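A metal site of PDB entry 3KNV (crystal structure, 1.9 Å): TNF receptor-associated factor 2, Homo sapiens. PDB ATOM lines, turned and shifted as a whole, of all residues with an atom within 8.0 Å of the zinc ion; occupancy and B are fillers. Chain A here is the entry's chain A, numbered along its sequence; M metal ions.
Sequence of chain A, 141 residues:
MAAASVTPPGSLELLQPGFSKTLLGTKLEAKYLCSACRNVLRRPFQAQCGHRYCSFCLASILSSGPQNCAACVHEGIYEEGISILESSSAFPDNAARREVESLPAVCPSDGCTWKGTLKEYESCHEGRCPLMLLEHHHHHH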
ATOM      1  N   VAL A 106       8.358  -0.781 -11.591  1.00  0.00           N
ATOM      2  CA  VAL A 106       9.131   0.219 -10.856  1.00  0.00           C
ATOM      3  C   VAL A 106      10.119   0.822 -11.847  1.00  0.00           C
ATOM      4  O   VAL A 106      10.650   0.104 -12.701  1.00  0.00           O
ATOM      5  CB  VAL A 106       9.901  -0.424  -9.678  1.00  0.00           C
ATOM      6  CG1 VAL A 106       8.929  -1.047  -8.704  1.00  0.00           C
ATOM      7  CG2 VAL A 106      10.879  -1.476 -10.196  1.00  0.00           C
ATOM      8  N   CYS A 107      10.357   2.127 -11.754  1.00  0.00           N
ATOM      9  CA  CYS A 107      11.286   2.760 -12.688  1.00  0.00           C
ATOM     10  C   CYS A 107      12.650   2.098 -12.651  1.00  0.00           C
ATOM     11  O   CYS A 107      13.174   1.791 -11.576  1.00  0.00           O
ATOM     12  CB  CYS A 107      11.443   4.255 -12.400  1.00  0.00           C
ATOM     13  SG  CYS A 107      12.598   5.042 -13.542  1.00  0.00           S
ATOM     14  N   PRO A 108      13.257   1.879 -13.819  1.00  0.00           N
ATOM     15  CA  PRO A 108      14.575   1.247 -13.899  1.00  0.00           C
ATOM     16  C   PRO A 108      15.729   2.156 -13.482  1.00  0.00           C
ATOM     17  O   PRO A 108      16.811   1.679 -13.141  1.00  0.00           O
ATOM     18  CB  PRO A 108      14.654   0.821 -15.361  1.00  0.00           C
ATOM     19  CG  PRO A 108      13.909   1.907 -16.056  1.00  0.00           C
ATOM     20  CD  PRO A 108      12.695   2.094 -15.175  1.00  0.00           C
ATOM     21  N   SER A 109      15.498   3.473 -13.501  1.00  0.00           N
ATOM     22  CA  SER A 109      16.539   4.426 -13.106  1.00  0.00           C
ATOM     23  C   SER A 109      17.000   4.156 -11.674  1.00  0.00           C
ATOM     24  O   SER A 109      16.217   4.257 -10.733  1.00  0.00           O
ATOM     25  CB  SER A 109      16.017   5.864 -13.229  1.00  0.00           C
ATOM     26  OG  SER A 109      15.734   6.203 -14.569  1.00  0.00           O
ATOM     27  N   ASP A 110      18.272   3.830 -11.519  1.00  0.00           N
ATOM     28  CA  ASP A 110      18.830   3.540 -10.206  1.00  0.00           C
ATOM     29  C   ASP A 110      18.732   4.760  -9.293  1.00  0.00           C
ATOM     30  O   ASP A 110      19.547   5.676  -9.367  1.00  0.00           O
ATOM     31  CB  ASP A 110      20.296   3.109 -10.328  1.00  0.00           C
ATOM     32  CG  ASP A 110      20.859   2.562  -9.033  1.00  0.00           C
ATOM     33  OD1 ASP A 110      20.351   1.529  -8.549  1.00  0.00           O
ATOM     34  OD2 ASP A 110      21.816   3.165  -8.493  1.00  0.00           O
ATOM     35  N   GLY A 111      17.713   4.769  -8.439  1.00  0.00           N
ATOM     36  CA  GLY A 111      17.529   5.889  -7.529  1.00  0.00           C
ATOM     37  C   GLY A 111      16.161   6.525  -7.619  1.00  0.00           C
ATOM     38  O   GLY A 111      15.871   7.469  -6.885  1.00  0.00           O
ATOM     39  N   CYS A 112      15.309   6.029  -8.514  1.00  0.00           N
ATOM     40  CA  CYS A 112      13.971   6.582  -8.657  1.00  0.00           C
ATOM     41  C   CYS A 112      12.965   5.780  -7.848  1.00  0.00           C
ATOM     42  O   CYS A 112      13.108   4.562  -7.708  1.00  0.00           O
ATOM     43  CB  CYS A 112      13.550   6.599 -10.128  1.00  0.00           C
ATOM     44  SG  CYS A 112      11.996   7.447 -10.397  1.00  0.00           S
ATOM     45  N   THR A 113      11.948   6.453  -7.329  1.00  0.00           N
ATOM     46  CA  THR A 113      10.923   5.799  -6.515  1.00  0.00           C
ATOM     47  C   THR A 113       9.587   5.607  -7.206  1.00  0.00           C
ATOM     48  O   THR A 113       8.644   5.085  -6.608  1.00  0.00           O
ATOM     49  CB  THR A 113      10.680   6.577  -5.215  1.00  0.00           C
ATOM     50  OG1 THR A 113      10.166   7.885  -5.523  1.00  0.00           O
ATOM     51  CG2 THR A 113      11.971   6.717  -4.413  1.00  0.00           C
ATOM     52  N   TRP A 114       9.487   6.016  -8.473  1.00  0.00           N
ATOM     53  CA  TRP A 114       8.236   5.872  -9.202  1.00  0.00           C
ATOM     54  C   TRP A 114       7.802   4.401  -9.266  1.00  0.00           C
ATOM     55  O   TRP A 114       8.608   3.520  -9.543  1.00  0.00           O
ATOM     56  CB  TRP A 114       8.368   6.410 -10.632  1.00  0.00           C
ATOM     57  CG  TRP A 114       7.064   6.379 -11.377  1.00  0.00           C
ATOM     58  CD1 TRP A 114       6.138   7.374 -11.457  1.00  0.00           C
ATOM     59  CD2 TRP A 114       6.498   5.251 -12.052  1.00  0.00           C
ATOM     60  NE1 TRP A 114       5.027   6.940 -12.134  1.00  0.00           N
ATOM     61  CE2 TRP A 114       5.219   5.639 -12.511  1.00  0.00           C
ATOM     62  CE3 TRP A 114       6.935   3.945 -12.317  1.00  0.00           C
ATOM     63  CZ2 TRP A 114       4.378   4.781 -13.224  1.00  0.00           C
ATOM     64  CZ3 TRP A 114       6.100   3.081 -13.019  1.00  0.00           C
ATOM     65  CH2 TRP A 114       4.832   3.508 -13.464  1.00  0.00           C
ATOM     66  N   LYS A 115       6.524   4.174  -9.005  1.00  0.00           N
ATOM     67  CA  LYS A 115       5.947   2.832  -9.038  1.00  0.00           C
ATOM     68  C   LYS A 115       4.537   2.865  -9.605  1.00  0.00           C
ATOM     69  O   LYS A 115       3.787   3.817  -9.385  1.00  0.00           O
ATOM     70  CB  LYS A 115       5.919   2.216  -7.640  1.00  0.00           C
ATOM     71  CG  LYS A 115       7.263   1.748  -7.121  1.00  0.00           C
ATOM     72  CD  LYS A 115       7.084   0.818  -5.920  1.00  0.00           C
ATOM     73  CE  LYS A 115       8.417   0.162  -5.538  1.00  0.00           C
ATOM     74  NZ  LYS A 115       8.241  -0.936  -4.555  1.00  0.00           N
ATOM     75  N   TYR A 121       3.734   3.270 -16.571  1.00  0.00           N
ATOM     76  CA  TYR A 121       5.131   3.591 -16.779  1.00  0.00           C
ATOM     77  C   TYR A 121       5.319   4.124 -18.193  1.00  0.00           C
ATOM     78  O   TYR A 121       5.910   5.183 -18.404  1.00  0.00           O
ATOM     79  CB  TYR A 121       6.003   2.356 -16.598  1.00  0.00           C
ATOM     80  CG  TYR A 121       7.449   2.621 -16.948  1.00  0.00           C
ATOM     81  CD1 TYR A 121       8.287   3.343 -16.089  1.00  0.00           C
ATOM     82  CD2 TYR A 121       7.981   2.193 -18.167  1.00  0.00           C
ATOM     83  CE1 TYR A 121       9.601   3.636 -16.434  1.00  0.00           C
ATOM     84  CE2 TYR A 121       9.297   2.487 -18.522  1.00  0.00           C
ATOM     85  CZ  TYR A 121      10.095   3.210 -17.654  1.00  0.00           C
ATOM     86  OH  TYR A 121      11.387   3.507 -18.006  1.00  0.00           O
ATOM     87  N   HIS A 125       5.429   7.787 -16.993  1.00  0.00           N
ATOM     88  CA  HIS A 125       6.770   8.020 -16.478  1.00  0.00           C
ATOM     89  C   HIS A 125       7.929   7.941 -17.469  1.00  0.00           C
ATOM     90  O   HIS A 125       8.842   8.764 -17.411  1.00  0.00           O
ATOM     91  CB  HIS A 125       7.051   7.077 -15.313  1.00  0.00           C
ATOM     92  CG  HIS A 125       8.212   7.506 -14.465  1.00  0.00           C
ATOM     93  ND1 HIS A 125       8.213   8.701 -13.784  1.00  0.00           N
ATOM     94  CD2 HIS A 125       9.401   6.912 -14.219  1.00  0.00           C
ATOM     95  CE1 HIS A 125       9.366   8.832 -13.146  1.00  0.00           C
ATOM     96  NE2 HIS A 125      10.098   7.761 -13.390  1.00  0.00           N
ATOM     97  N   GLU A 126       7.906   6.961 -18.365  1.00  0.00           N
ATOM     98  CA  GLU A 126       8.999   6.823 -19.322  1.00  0.00           C
ATOM     99  C   GLU A 126       9.199   8.130 -20.072  1.00  0.00           C
ATOM    100  O   GLU A 126       8.250   8.727 -20.562  1.00  0.00           O
ATOM    101  CB  GLU A 126       8.716   5.695 -20.313  1.00  0.00           C
ATOM    102  CG  GLU A 126       9.956   5.261 -21.081  1.00  0.00           C
ATOM    103  CD  GLU A 126       9.705   4.085 -22.000  1.00  0.00           C
ATOM    104  OE1 GLU A 126      10.665   3.343 -22.275  1.00  0.00           O
ATOM    105  OE2 GLU A 126       8.545   3.912 -22.453  1.00  0.00           O
ATOM    106  N   GLY A 127      10.452   8.585 -20.144  1.00  0.00           N
ATOM    107  CA  GLY A 127      10.754   9.833 -20.823  1.00  0.00           C
ATOM    108  C   GLY A 127      10.498  11.047 -19.955  1.00  0.00           C
ATOM    109  O   GLY A 127      10.692  12.189 -20.394  1.00  0.00           O
ATOM    110  N   ARG A 128      10.064  10.816 -18.726  1.00  0.00           N
ATOM    111  CA  ARG A 128       9.773  11.892 -17.784  1.00  0.00           C
ATOM    112  C   ARG A 128      10.389  11.578 -16.423  1.00  0.00           C
ATOM    113  O   ARG A 128       9.891  12.030 -15.391  1.00  0.00           O
ATOM    114  CB  ARG A 128       8.253  12.044 -17.613  1.00  0.00           C
ATOM    115  CG  ARG A 128       7.482  12.301 -18.894  1.00  0.00           C
ATOM    116  CD  ARG A 128       5.990  12.261 -18.652  1.00  0.00           C
ATOM    117  NE  ARG A 128       5.220  12.362 -19.890  1.00  0.00           N
ATOM    118  CZ  ARG A 128       5.123  13.465 -20.619  1.00  0.00           C
ATOM    119  NH1 ARG A 128       5.722  14.576 -20.235  1.00  0.00           N
ATOM    120  NH2 ARG A 128       4.413  13.453 -21.735  1.00  0.00           N
ATOM    121  N   CYS A 129      11.480  10.820 -16.442  1.00  0.00           N
ATOM    122  CA  CYS A 129      12.166  10.432 -15.206  1.00  0.00           C
ATOM    123  C   CYS A 129      13.158  11.470 -14.690  1.00  0.00           C
ATOM    124  O   CYS A 129      14.056  11.901 -15.414  1.00  0.00           O
ATOM    125  CB  CYS A 129      12.891   9.098 -15.389  1.00  0.00           C
ATOM    126  SG  CYS A 129      13.826   8.596 -13.936  1.00  0.00           S
ATOM    127  N   PRO A 130      13.026  11.857 -13.409  1.00  0.00           N
ATOM    128  CA  PRO A 130      13.887  12.832 -12.732  1.00  0.00           C
ATOM    129  C   PRO A 130      15.372  12.506 -12.828  1.00  0.00           C
ATOM    130  O   PRO A 130      16.195  13.378 -13.087  1.00  0.00           O
ATOM    131  CB  PRO A 130      13.382  12.794 -11.295  1.00  0.00           C
ATOM    132  CG  PRO A 130      11.940  12.476 -11.454  1.00  0.00           C
ATOM    133  CD  PRO A 130      11.955  11.401 -12.505  1.00  0.00           C
ATOM    134  N   LEU A 131      15.710  11.237 -12.612  1.00  0.00           N
ATOM    135  CA  LEU A 131      17.112  10.800 -12.659  1.00  0.00           C
ATOM    136  C   LEU A 131      17.719  10.965 -14.037  1.00  0.00           C
ATOM    137  O   LEU A 131      18.939  11.038 -14.179  1.00  0.00           O
ATOM    138  CB  LEU A 131      17.216   9.332 -12.228  1.00  0.00           C
ATOM    139  CG  LEU A 131      17.087   9.013 -10.735  1.00  0.00           C
ATOM    140  CD1 LEU A 131      18.287   9.572 -10.002  1.00  0.00           C
ATOM    141  CD2 LEU A 131      15.796   9.587 -10.190  1.00  0.00           C
ATOM    142  N   MET A 132      16.868  11.007 -15.058  1.00  0.00           N
ATOM    143  CA  MET A 132      17.338  11.142 -16.433  1.00  0.00           C
ATOM    144  C   MET A 132      17.349  12.582 -16.935  1.00  0.00           C
ATOM    145  O   MET A 132      18.261  12.987 -17.644  1.00  0.00           O
ATOM    146  CB  MET A 132      16.462  10.303 -17.374  1.00  0.00           C
ATOM    147  CG  MET A 132      16.443   8.809 -17.072  1.00  0.00           C
ATOM    148  SD  MET A 132      18.075   8.065 -17.114  1.00  0.00           S
ATOM    149  CE  MET A 132      18.353   7.964 -18.875  1.00  0.00           C
HETATM  150 ZN    ZN M   1      12.135   7.304 -12.852  1.00  0.00          ZN
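The side-chain sulfur (SG) of Cys 129 lies close to the backbone NH (N) of Leu 131, at 3.5 Å. OG of Ser 109 sits close to SG of Cys 129, 3.1 Å away. The side-chain sulfur (SG) of Cys 107 sits close to the backbone NH (N) of Ser 109 (3.3 Å). The side-chain sulfur (SG) of Cys 112 lies close to the backbone NH (N) of Trp 114, at 3.5 Å. The backbone NH (N) of Cys 107 sits at hydrogen-bond distance from the backbone carbonyl oxygen (O) of Trp 114, 3.1 Å away.
Of the 19 residues printed, 4 come within 4 Å of the zinc ion.
The zinc ion is bound by NE2 of His 125 (2.2 Å). SG of Cys 129 is bound to the zinc ion (2.4 Å). SG of Cys 107 binds the zinc ion (2.4 Å). The zinc ion is bound by SG of Cys 112 (2.5 Å).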
